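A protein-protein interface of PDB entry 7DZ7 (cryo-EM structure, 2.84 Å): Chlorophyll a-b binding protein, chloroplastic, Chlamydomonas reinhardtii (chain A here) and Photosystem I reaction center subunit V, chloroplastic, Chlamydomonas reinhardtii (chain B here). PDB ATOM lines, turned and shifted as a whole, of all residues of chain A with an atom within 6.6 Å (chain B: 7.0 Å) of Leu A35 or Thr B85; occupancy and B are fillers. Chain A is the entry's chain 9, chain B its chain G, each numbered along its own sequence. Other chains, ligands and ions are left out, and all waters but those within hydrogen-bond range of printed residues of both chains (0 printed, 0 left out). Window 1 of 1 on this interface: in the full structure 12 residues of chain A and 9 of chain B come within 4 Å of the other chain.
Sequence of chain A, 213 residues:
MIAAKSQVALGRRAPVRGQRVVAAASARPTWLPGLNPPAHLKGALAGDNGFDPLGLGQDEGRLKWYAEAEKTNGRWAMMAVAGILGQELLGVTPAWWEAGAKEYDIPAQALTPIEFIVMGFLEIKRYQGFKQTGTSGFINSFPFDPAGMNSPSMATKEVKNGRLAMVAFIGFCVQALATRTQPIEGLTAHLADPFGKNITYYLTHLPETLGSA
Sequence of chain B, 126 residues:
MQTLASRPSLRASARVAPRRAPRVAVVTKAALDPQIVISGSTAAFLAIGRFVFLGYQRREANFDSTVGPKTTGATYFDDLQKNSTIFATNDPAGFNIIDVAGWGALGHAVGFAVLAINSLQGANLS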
ATOM      1  N   ARG A  28      -2.957 -12.212  32.941  1.00  0.00           N
ATOM      2  CA  ARG A  28      -3.157 -13.655  32.894  1.00  0.00           C
ATOM      3  C   ARG A  28      -3.288 -14.139  31.454  1.00  0.00           C
ATOM      4  O   ARG A  28      -3.800 -13.416  30.603  1.00  0.00           O
ATOM      5  CB  ARG A  28      -4.404 -14.048  33.682  1.00  0.00           C
ATOM      6  CG  ARG A  28      -4.394 -13.583  35.120  1.00  0.00           C
ATOM      7  CD  ARG A  28      -5.520 -14.218  35.919  1.00  0.00           C
ATOM      8  NE  ARG A  28      -6.775 -14.272  35.173  1.00  0.00           N
ATOM      9  CZ  ARG A  28      -7.594 -13.239  35.016  1.00  0.00           C
ATOM     10  NH1 ARG A  28      -8.717 -13.381  34.331  1.00  0.00           N
ATOM     11  NH2 ARG A  28      -7.288 -12.058  35.533  1.00  0.00           N
ATOM     12  N   THR A  30      -5.209 -15.723  28.702  1.00  0.00           N
ATOM     13  CA  THR A  30      -6.640 -15.869  28.500  1.00  0.00           C
ATOM     14  C   THR A  30      -6.912 -16.788  27.318  1.00  0.00           C
ATOM     15  O   THR A  30      -6.036 -17.069  26.497  1.00  0.00           O
ATOM     16  CB  THR A  30      -7.296 -14.502  28.284  1.00  0.00           C
ATOM     17  OG1 THR A  30      -6.710 -13.861  27.145  1.00  0.00           O
ATOM     18  CG2 THR A  30      -7.107 -13.625  29.508  1.00  0.00           C
ATOM     19  N   TRP A  31      -8.159 -17.251  27.236  1.00  0.00           N
ATOM     20  CA  TRP A  31      -8.520 -18.259  26.248  1.00  0.00           C
ATOM     21  C   TRP A  31      -8.447 -17.737  24.819  1.00  0.00           C
ATOM     22  O   TRP A  31      -8.331 -18.541  23.891  1.00  0.00           O
ATOM     23  CB  TRP A  31      -9.919 -18.800  26.537  1.00  0.00           C
ATOM     24  CG  TRP A  31     -11.006 -17.781  26.470  1.00  0.00           C
ATOM     25  CD1 TRP A  31     -11.264 -16.800  27.375  1.00  0.00           C
ATOM     26  CD2 TRP A  31     -11.997 -17.653  25.447  1.00  0.00           C
ATOM     27  NE1 TRP A  31     -12.350 -16.064  26.979  1.00  0.00           N
ATOM     28  CE2 TRP A  31     -12.819 -16.569  25.796  1.00  0.00           C
ATOM     29  CE3 TRP A  31     -12.267 -18.350  24.268  1.00  0.00           C
ATOM     30  CZ2 TRP A  31     -13.888 -16.161  25.010  1.00  0.00           C
ATOM     31  CZ3 TRP A  31     -13.328 -17.946  23.491  1.00  0.00           C
ATOM     32  CH2 TRP A  31     -14.127 -16.862  23.863  1.00  0.00           C
ATOM     33  N   LEU A  32      -8.514 -16.423  24.619  1.00  0.00           N
ATOM     34  CA  LEU A  32      -8.302 -15.845  23.307  1.00  0.00           C
ATOM     35  C   LEU A  32      -7.068 -14.951  23.331  1.00  0.00           C
ATOM     36  O   LEU A  32      -6.874 -14.200  24.293  1.00  0.00           O
ATOM     37  CB  LEU A  32      -9.514 -15.019  22.846  1.00  0.00           C
ATOM     38  CG  LEU A  32     -10.631 -15.723  22.072  1.00  0.00           C
ATOM     39  CD1 LEU A  32     -11.745 -14.742  21.775  1.00  0.00           C
ATOM     40  CD2 LEU A  32     -10.123 -16.335  20.781  1.00  0.00           C
ATOM     41  N   PRO A  33      -6.222 -14.998  22.301  1.00  0.00           N
ATOM     42  CA  PRO A  33      -5.041 -14.125  22.291  1.00  0.00           C
ATOM     43  C   PRO A  33      -5.448 -12.663  22.214  1.00  0.00           C
ATOM     44  O   PRO A  33      -6.315 -12.284  21.424  1.00  0.00           O
ATOM     45  CB  PRO A  33      -4.279 -14.568  21.037  1.00  0.00           C
ATOM     46  CG  PRO A  33      -4.816 -15.910  20.709  1.00  0.00           C
ATOM     47  CD  PRO A  33      -6.240 -15.887  21.130  1.00  0.00           C
ATOM     48  N   GLY A  34      -4.814 -11.841  23.047  1.00  0.00           N
ATOM     49  CA  GLY A  34      -5.103 -10.423  23.053  1.00  0.00           C
ATOM     50  C   GLY A  34      -6.430 -10.048  23.668  1.00  0.00           C
ATOM     51  O   GLY A  34      -6.850  -8.895  23.540  1.00  0.00           O
ATOM     52  N   LEU A  35      -7.101 -10.983  24.332  1.00  0.00           N
ATOM     53  CA  LEU A  35      -8.423 -10.742  24.892  1.00  0.00           C
ATOM     54  C   LEU A  35      -8.317 -10.283  26.339  1.00  0.00           C
ATOM     55  O   LEU A  35      -7.561 -10.858  27.129  1.00  0.00           O
ATOM     56  CB  LEU A  35      -9.275 -12.006  24.805  1.00  0.00           C
ATOM     57  CG  LEU A  35     -10.594 -11.983  25.579  1.00  0.00           C
ATOM     58  CD1 LEU A  35     -11.735 -12.479  24.717  1.00  0.00           C
ATOM     59  CD2 LEU A  35     -10.479 -12.822  26.838  1.00  0.00           C
ATOM     60  N   ASN A  36      -9.075  -9.251  26.677  1.00  0.00           N
ATOM     61  CA  ASN A  36      -9.198  -8.821  28.062  1.00  0.00           C
ATOM     62  C   ASN A  36     -10.265  -9.658  28.762  1.00  0.00           C
ATOM     63  O   ASN A  36     -11.350  -9.853  28.207  1.00  0.00           O
ATOM     64  CB  ASN A  36      -9.565  -7.344  28.135  1.00  0.00           C
ATOM     65  CG  ASN A  36      -9.623  -6.826  29.559  1.00  0.00           C
ATOM     66  OD1 ASN A  36     -10.694  -6.742  30.160  1.00  0.00           O
ATOM     67  ND2 ASN A  36      -8.468  -6.477  30.108  1.00  0.00           N
ATOM     68  N   PRO A  37     -10.002 -10.167  29.961  1.00  0.00           N
ATOM     69  CA  PRO A  37     -10.999 -10.990  30.645  1.00  0.00           C
ATOM     70  C   PRO A  37     -12.160 -10.144  31.133  1.00  0.00           C
ATOM     71  O   PRO A  37     -11.994  -8.946  31.408  1.00  0.00           O
ATOM     72  CB  PRO A  37     -10.214 -11.596  31.815  1.00  0.00           C
ATOM     73  CG  PRO A  37      -9.109 -10.646  32.056  1.00  0.00           C
ATOM     74  CD  PRO A  37      -8.743 -10.090  30.720  1.00  0.00           C
ATOM     75  N   PRO A  38     -13.351 -10.724  31.255  1.00  0.00           N
ATOM     76  CA  PRO A  38     -14.506  -9.946  31.708  1.00  0.00           C
ATOM     77  C   PRO A  38     -14.315  -9.439  33.130  1.00  0.00           C
ATOM     78  O   PRO A  38     -13.364  -9.785  33.831  1.00  0.00           O
ATOM     79  CB  PRO A  38     -15.671 -10.935  31.607  1.00  0.00           C
ATOM     80  CG  PRO A  38     -15.042 -12.278  31.576  1.00  0.00           C
ATOM     81  CD  PRO A  38     -13.729 -12.100  30.896  1.00  0.00           C
ATOM     82  N   HIS A  40     -16.437  -9.681  35.856  1.00  0.00           N
ATOM     83  CA  HIS A  40     -16.815 -10.578  36.937  1.00  0.00           C
ATOM     84  C   HIS A  40     -15.803 -11.691  37.157  1.00  0.00           C
ATOM     85  O   HIS A  40     -15.893 -12.393  38.169  1.00  0.00           O
ATOM     86  CB  HIS A  40     -18.184 -11.188  36.652  1.00  0.00           C
ATOM     87  CG  HIS A  40     -18.201 -12.091  35.463  1.00  0.00           C
ATOM     88  ND1 HIS A  40     -18.170 -11.617  34.169  1.00  0.00           N
ATOM     89  CD2 HIS A  40     -18.237 -13.439  35.369  1.00  0.00           C
ATOM     90  CE1 HIS A  40     -18.190 -12.637  33.330  1.00  0.00           C
ATOM     91  NE2 HIS A  40     -18.229 -13.753  34.034  1.00  0.00           N
ATOM     92  N   ASN A  49      -9.142 -18.300  33.487  1.00  0.00           N
ATOM     93  CA  ASN A  49      -8.482 -17.912  32.248  1.00  0.00           C
ATOM     94  C   ASN A  49      -9.359 -16.951  31.455  1.00  0.00           C
ATOM     95  O   ASN A  49      -9.229 -16.839  30.236  1.00  0.00           O
ATOM     96  CB  ASN A  49      -8.138 -19.141  31.415  1.00  0.00           C
ATOM     97  CG  ASN A  49      -7.196 -20.081  32.126  1.00  0.00           C
ATOM     98  OD1 ASN A  49      -6.384 -19.663  32.951  1.00  0.00           O
ATOM     99  ND2 ASN A  49      -7.292 -21.361  31.807  1.00  0.00           N
ATOM    100  N   GLY A  50     -10.264 -16.260  32.144  1.00  0.00           N
ATOM    101  CA  GLY A  50     -11.150 -15.319  31.492  1.00  0.00           C
ATOM    102  C   GLY A  50     -12.169 -15.947  30.575  1.00  0.00           C
ATOM    103  O   GLY A  50     -12.613 -15.300  29.624  1.00  0.00           O
ATOM    104  N   PHE A  51     -12.560 -17.191  30.834  1.00  0.00           N
ATOM    105  CA  PHE A  51     -13.443 -17.941  29.945  1.00  0.00           C
ATOM    106  C   PHE A  51     -14.860 -17.914  30.513  1.00  0.00           C
ATOM    107  O   PHE A  51     -15.259 -18.779  31.290  1.00  0.00           O
ATOM    108  CB  PHE A  51     -12.931 -19.364  29.767  1.00  0.00           C
ATOM    109  CG  PHE A  51     -13.723 -20.178  28.793  1.00  0.00           C
ATOM    110  CD1 PHE A  51     -13.803 -19.805  27.468  1.00  0.00           C
ATOM    111  CD2 PHE A  51     -14.375 -21.323  29.198  1.00  0.00           C
ATOM    112  CE1 PHE A  51     -14.527 -20.553  26.572  1.00  0.00           C
ATOM    113  CE2 PHE A  51     -15.098 -22.073  28.300  1.00  0.00           C
ATOM    114  CZ  PHE A  51     -15.173 -21.686  26.988  1.00  0.00           C
ATOM    115  N   ASP A  52     -15.622 -16.894  30.116  1.00  0.00           N
ATOM    116  CA  ASP A  52     -17.054 -16.822  30.405  1.00  0.00           C
ATOM    117  C   ASP A  52     -17.735 -16.109  29.247  1.00  0.00           C
ATOM    118  O   ASP A  52     -18.349 -15.050  29.414  1.00  0.00           O
ATOM    119  CB  ASP A  52     -17.310 -16.107  31.730  1.00  0.00           C
ATOM    120  CG  ASP A  52     -18.728 -16.298  32.240  1.00  0.00           C
ATOM    121  OD1 ASP A  52     -19.582 -16.800  31.491  1.00  0.00           O
ATOM    122  OD2 ASP A  52     -18.987 -15.949  33.411  1.00  0.00           O
ATOM    123  N   PRO A  53     -17.648 -16.678  28.043  1.00  0.00           N
ATOM    124  CA  PRO A  53     -18.190 -15.979  26.871  1.00  0.00           C
ATOM    125  C   PRO A  53     -19.694 -15.810  26.922  1.00  0.00           C
ATOM    126  O   PRO A  53     -20.216 -14.844  26.354  1.00  0.00           O
ATOM    127  CB  PRO A  53     -17.756 -16.874  25.704  1.00  0.00           C
ATOM    128  CG  PRO A  53     -17.585 -18.211  26.297  1.00  0.00           C
ATOM    129  CD  PRO A  53     -17.121 -18.006  27.699  1.00  0.00           C
ATOM    130  N   LEU A  54     -20.407 -16.717  27.585  1.00  0.00           N
ATOM    131  CA  LEU A  54     -21.831 -16.531  27.808  1.00  0.00           C
ATOM    132  C   LEU A  54     -22.115 -15.555  28.938  1.00  0.00           C
ATOM    133  O   LEU A  54     -23.212 -14.991  28.991  1.00  0.00           O
ATOM    134  CB  LEU A  54     -22.497 -17.871  28.127  1.00  0.00           C
ATOM    135  CG  LEU A  54     -22.654 -18.934  27.040  1.00  0.00           C
ATOM    136  CD1 LEU A  54     -23.812 -19.849  27.392  1.00  0.00           C
ATOM    137  CD2 LEU A  54     -22.857 -18.338  25.673  1.00  0.00           C
ATOM    138  N   GLY A  55     -21.156 -15.340  29.830  1.00  0.00           N
ATOM    139  CA  GLY A  55     -21.379 -14.486  30.978  1.00  0.00           C
ATOM    140  C   GLY A  55     -22.215 -15.140  32.051  1.00  0.00           C
ATOM    141  O   GLY A  55     -23.016 -14.464  32.709  1.00  0.00           O
ATOM    142  N   LYS B  82     -25.920  -7.785  28.603  1.00  0.00           N
ATOM    143  CA  LYS B  82     -24.771  -6.980  28.237  1.00  0.00           C
ATOM    144  C   LYS B  82     -23.720  -7.837  27.542  1.00  0.00           C
ATOM    145  O   LYS B  82     -23.686  -9.061  27.680  1.00  0.00           O
ATOM    146  CB  LYS B  82     -24.154  -6.325  29.473  1.00  0.00           C
ATOM    147  CG  LYS B  82     -25.047  -5.324  30.180  1.00  0.00           C
ATOM    148  CD  LYS B  82     -24.411  -4.860  31.479  1.00  0.00           C
ATOM    149  CE  LYS B  82     -25.333  -3.959  32.273  1.00  0.00           C
ATOM    150  NZ  LYS B  82     -25.323  -2.561  31.770  1.00  0.00           N
ATOM    151  N   ASN B  83     -22.852  -7.172  26.784  1.00  0.00           N
ATOM    152  CA  ASN B  83     -21.706  -7.831  26.162  1.00  0.00           C
ATOM    153  C   ASN B  83     -20.646  -8.020  27.235  1.00  0.00           C
ATOM    154  O   ASN B  83     -19.752  -7.192  27.415  1.00  0.00           O
ATOM    155  CB  ASN B  83     -21.178  -7.016  24.990  1.00  0.00           C
ATOM    156  CG  ASN B  83     -22.251  -6.694  23.976  1.00  0.00           C
ATOM    157  OD1 ASN B  83     -23.407  -6.458  24.329  1.00  0.00           O
ATOM    158  ND2 ASN B  83     -21.876  -6.680  22.704  1.00  0.00           N
ATOM    159  N   SER B  84     -20.745  -9.136  27.958  1.00  0.00           N
ATOM    160  CA  SER B  84     -19.821  -9.386  29.055  1.00  0.00           C
ATOM    161  C   SER B  84     -18.399  -9.595  28.556  1.00  0.00           C
ATOM    162  O   SER B  84     -17.441  -9.356  29.299  1.00  0.00           O
ATOM    163  CB  SER B  84     -20.276 -10.603  29.857  1.00  0.00           C
ATOM    164  OG  SER B  84     -19.919 -10.478  31.220  1.00  0.00           O
ATOM    165  N   THR B  85     -18.242 -10.033  27.310  1.00  0.00           N
ATOM    166  CA  THR B  85     -16.936 -10.382  26.764  1.00  0.00           C
ATOM    167  C   THR B  85     -16.827  -9.801  25.362  1.00  0.00           C
ATOM    168  O   THR B  85     -17.423 -10.332  24.422  1.00  0.00           O
ATOM    169  CB  THR B  85     -16.746 -11.898  26.734  1.00  0.00           C
ATOM    170  OG1 THR B  85     -17.198 -12.461  27.972  1.00  0.00           O
ATOM    171  CG2 THR B  85     -15.288 -12.255  26.511  1.00  0.00           C
ATOM    172  N   ILE B  86     -16.070  -8.719  25.222  1.00  0.00           N
ATOM    173  CA  ILE B  86     -15.751  -8.194  23.900  1.00  0.00           C
ATOM    174  C   ILE B  86     -14.655  -9.055  23.298  1.00  0.00           C
ATOM    175  O   ILE B  86     -13.582  -9.228  23.892  1.00  0.00           O
ATOM    176  CB  ILE B  86     -15.330  -6.717  23.974  1.00  0.00           C
ATOM    177  CG1 ILE B  86     -14.079  -6.542  24.836  1.00  0.00           C
ATOM    178  CG2 ILE B  86     -16.464  -5.874  24.526  1.00  0.00           C
ATOM    179  CD1 ILE B  86     -13.494  -5.147  24.769  1.00  0.00           C
ATOM    180  N   PHE B  87     -14.921  -9.606  22.120  1.00  0.00           N
ATOM    181  CA  PHE B  87     -14.031 -10.585  21.503  1.00  0.00           C
ATOM    182  C   PHE B  87     -12.959  -9.829  20.735  1.00  0.00           C
ATOM    183  O   PHE B  87     -13.093  -9.543  19.546  1.00  0.00           O
ATOM    184  CB  PHE B  87     -14.826 -11.530  20.619  1.00  0.00           C
ATOM    185  CG  PHE B  87     -15.816 -12.359  21.380  1.00  0.00           C
ATOM    186  CD1 PHE B  87     -15.448 -13.576  21.917  1.00  0.00           C
ATOM    187  CD2 PHE B  87     -17.104 -11.905  21.585  1.00  0.00           C
ATOM    188  CE1 PHE B  87     -16.351 -14.335  22.625  1.00  0.00           C
ATOM    189  CE2 PHE B  87     -18.011 -12.661  22.295  1.00  0.00           C
ATOM    190  CZ  PHE B  87     -17.633 -13.875  22.816  1.00  0.00           C
ATOM    191  N   ALA B  88     -11.881  -9.500  21.437  1.00  0.00           N
ATOM    192  CA  ALA B  88     -10.780  -8.779  20.822  1.00  0.00           C
ATOM    193  C   ALA B  88     -10.067  -9.668  19.815  1.00  0.00           C
ATOM    194  O   ALA B  88      -9.938 -10.880  20.009  1.00  0.00           O
ATOM    195  CB  ALA B  88      -9.798  -8.301  21.888  1.00  0.00           C
ATOM    196  N   THR B  89      -9.603  -9.056  18.731  1.00  0.00           N
ATOM    197  CA  THR B  89      -8.924  -9.773  17.666  1.00  0.00           C
ATOM    198  C   THR B  89      -7.758  -8.936  17.174  1.00  0.00           C
ATOM    199  O   THR B  89      -7.887  -7.721  16.997  1.00  0.00           O
ATOM    200  CB  THR B  89      -9.871 -10.081  16.500  1.00  0.00           C
ATOM    201  OG1 THR B  89      -9.117 -10.581  15.389  1.00  0.00           O
ATOM    202  CG2 THR B  89     -10.614  -8.832  16.072  1.00  0.00           C
ATOM    203  N   ASN B  90      -6.625  -9.590  16.953  1.00  0.00           N
ATOM    204  CA  ASN B  90      -5.471  -8.931  16.367  1.00  0.00           C
ATOM    205  C   ASN B  90      -5.566  -8.849  14.851  1.00  0.00           C
ATOM    206  O   ASN B  90      -4.620  -8.387  14.206  1.00  0.00           O
ATOM    207  CB  ASN B  90      -4.189  -9.659  16.773  1.00  0.00           C
ATOM    208  CG  ASN B  90      -4.179 -10.044  18.236  1.00  0.00           C
ATOM    209  OD1 ASN B  90      -4.588  -9.266  19.097  1.00  0.00           O
ATOM    210  ND2 ASN B  90      -3.717 -11.252  18.525  1.00  0.00           N
ATOM    211  N   ILE B  97     -13.911 -14.176  16.201  1.00  0.00           N
ATOM    212  CA  ILE B  97     -14.456 -15.521  16.052  1.00  0.00           C
ATOM    213  C   ILE B  97     -15.944 -15.503  15.756  1.00  0.00           C
ATOM    214  O   ILE B  97     -16.485 -16.512  15.297  1.00  0.00           O
ATOM    215  CB  ILE B  97     -14.209 -16.385  17.303  1.00  0.00           C
ATOM    216  CG1 ILE B  97     -14.405 -15.572  18.581  1.00  0.00           C
ATOM    217  CG2 ILE B  97     -12.830 -16.993  17.263  1.00  0.00           C
ATOM    218  CD1 ILE B  97     -14.674 -16.421  19.791  1.00  0.00           C
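O of Asp A52 is in hydrogen-bond range of OG1 of Thr B85.
Of the printed residues of chain B, Leu A32 touches Phe B87 (3.9 Å) and Ile B97 (3.9 Å).
Of chain B, only Ala B88 comes within 4 Å of Gly A34.
Printed residues of chain B within 4 Å of Leu A35: Thr B85 (3.99 Å) and Ile B86 (3.8 Å).
Of the printed residues of chain A, Thr B85 touches Leu A35 (3.99 Å), Asp A52 (3.2 Å) and Pro A53 (3.8 Å).
Printed residues of chain A within 4 Å of Phe B87: Trp A31 (3.6 Å) and Leu A32 (3.9 Å).
Thr B89 touches none of the printed residues of chain A.
The nearest printed residue of chain A that does not touch Phe B87 is Pro A53 (4.2 Å).
NE1 of Trp A31 is in hydrogen-bond range of O of Gly A50, at 2.8 Å.
A ring nitrogen (NE2) of His A40 sits at hydrogen-bond distance from the side-chain carboxylate of Asp A52, 2.4 Å away.
N of Trp A31 is in hydrogen-bond range of O of Asn A49 (3.2 Å).
O of Leu A35 sits at hydrogen-bond distance from OG1 of Thr A30 (3.1 Å).
The side-chain hydroxyl of Thr A30 is in hydrogen-bond range of the backbone carbonyl oxygen of Leu A32.
The side-chain carboxylate (OD1) of Asp A52 lies within hydrogen-bond range of the backbone NH (N) of Gly A55.
Of the 10 printed residues of chain B, 6 touch a printed residue of chain A.
Hydrophobic or aromatic side chains of chain B within 4 Å of the printed part of chain A: Phe B87, Ala B88 and Ile B97.
Hydrophobic or aromatic side chains of chain A within 4 Å of the printed part of chain B: Trp A31, Leu A32, Leu A35, Pro A38 and His A40.
Among the printed residues, no Asp or Glu carboxylate lies within 4 Å of a Lys or Arg side-chain nitrogen of the other chain.
Among the printed residues, merely in contact across the chains: Trp A31 with Phe B87, Leu A32 with Phe B87, Leu A32 with Ile B97, Gly A34 with Ala B88, Leu A35 with Thr B85, Leu A35 with Ile B86, Pro A38 with Ser B84, His A40 with Ser B84 and Pro A53 with Thr B85.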
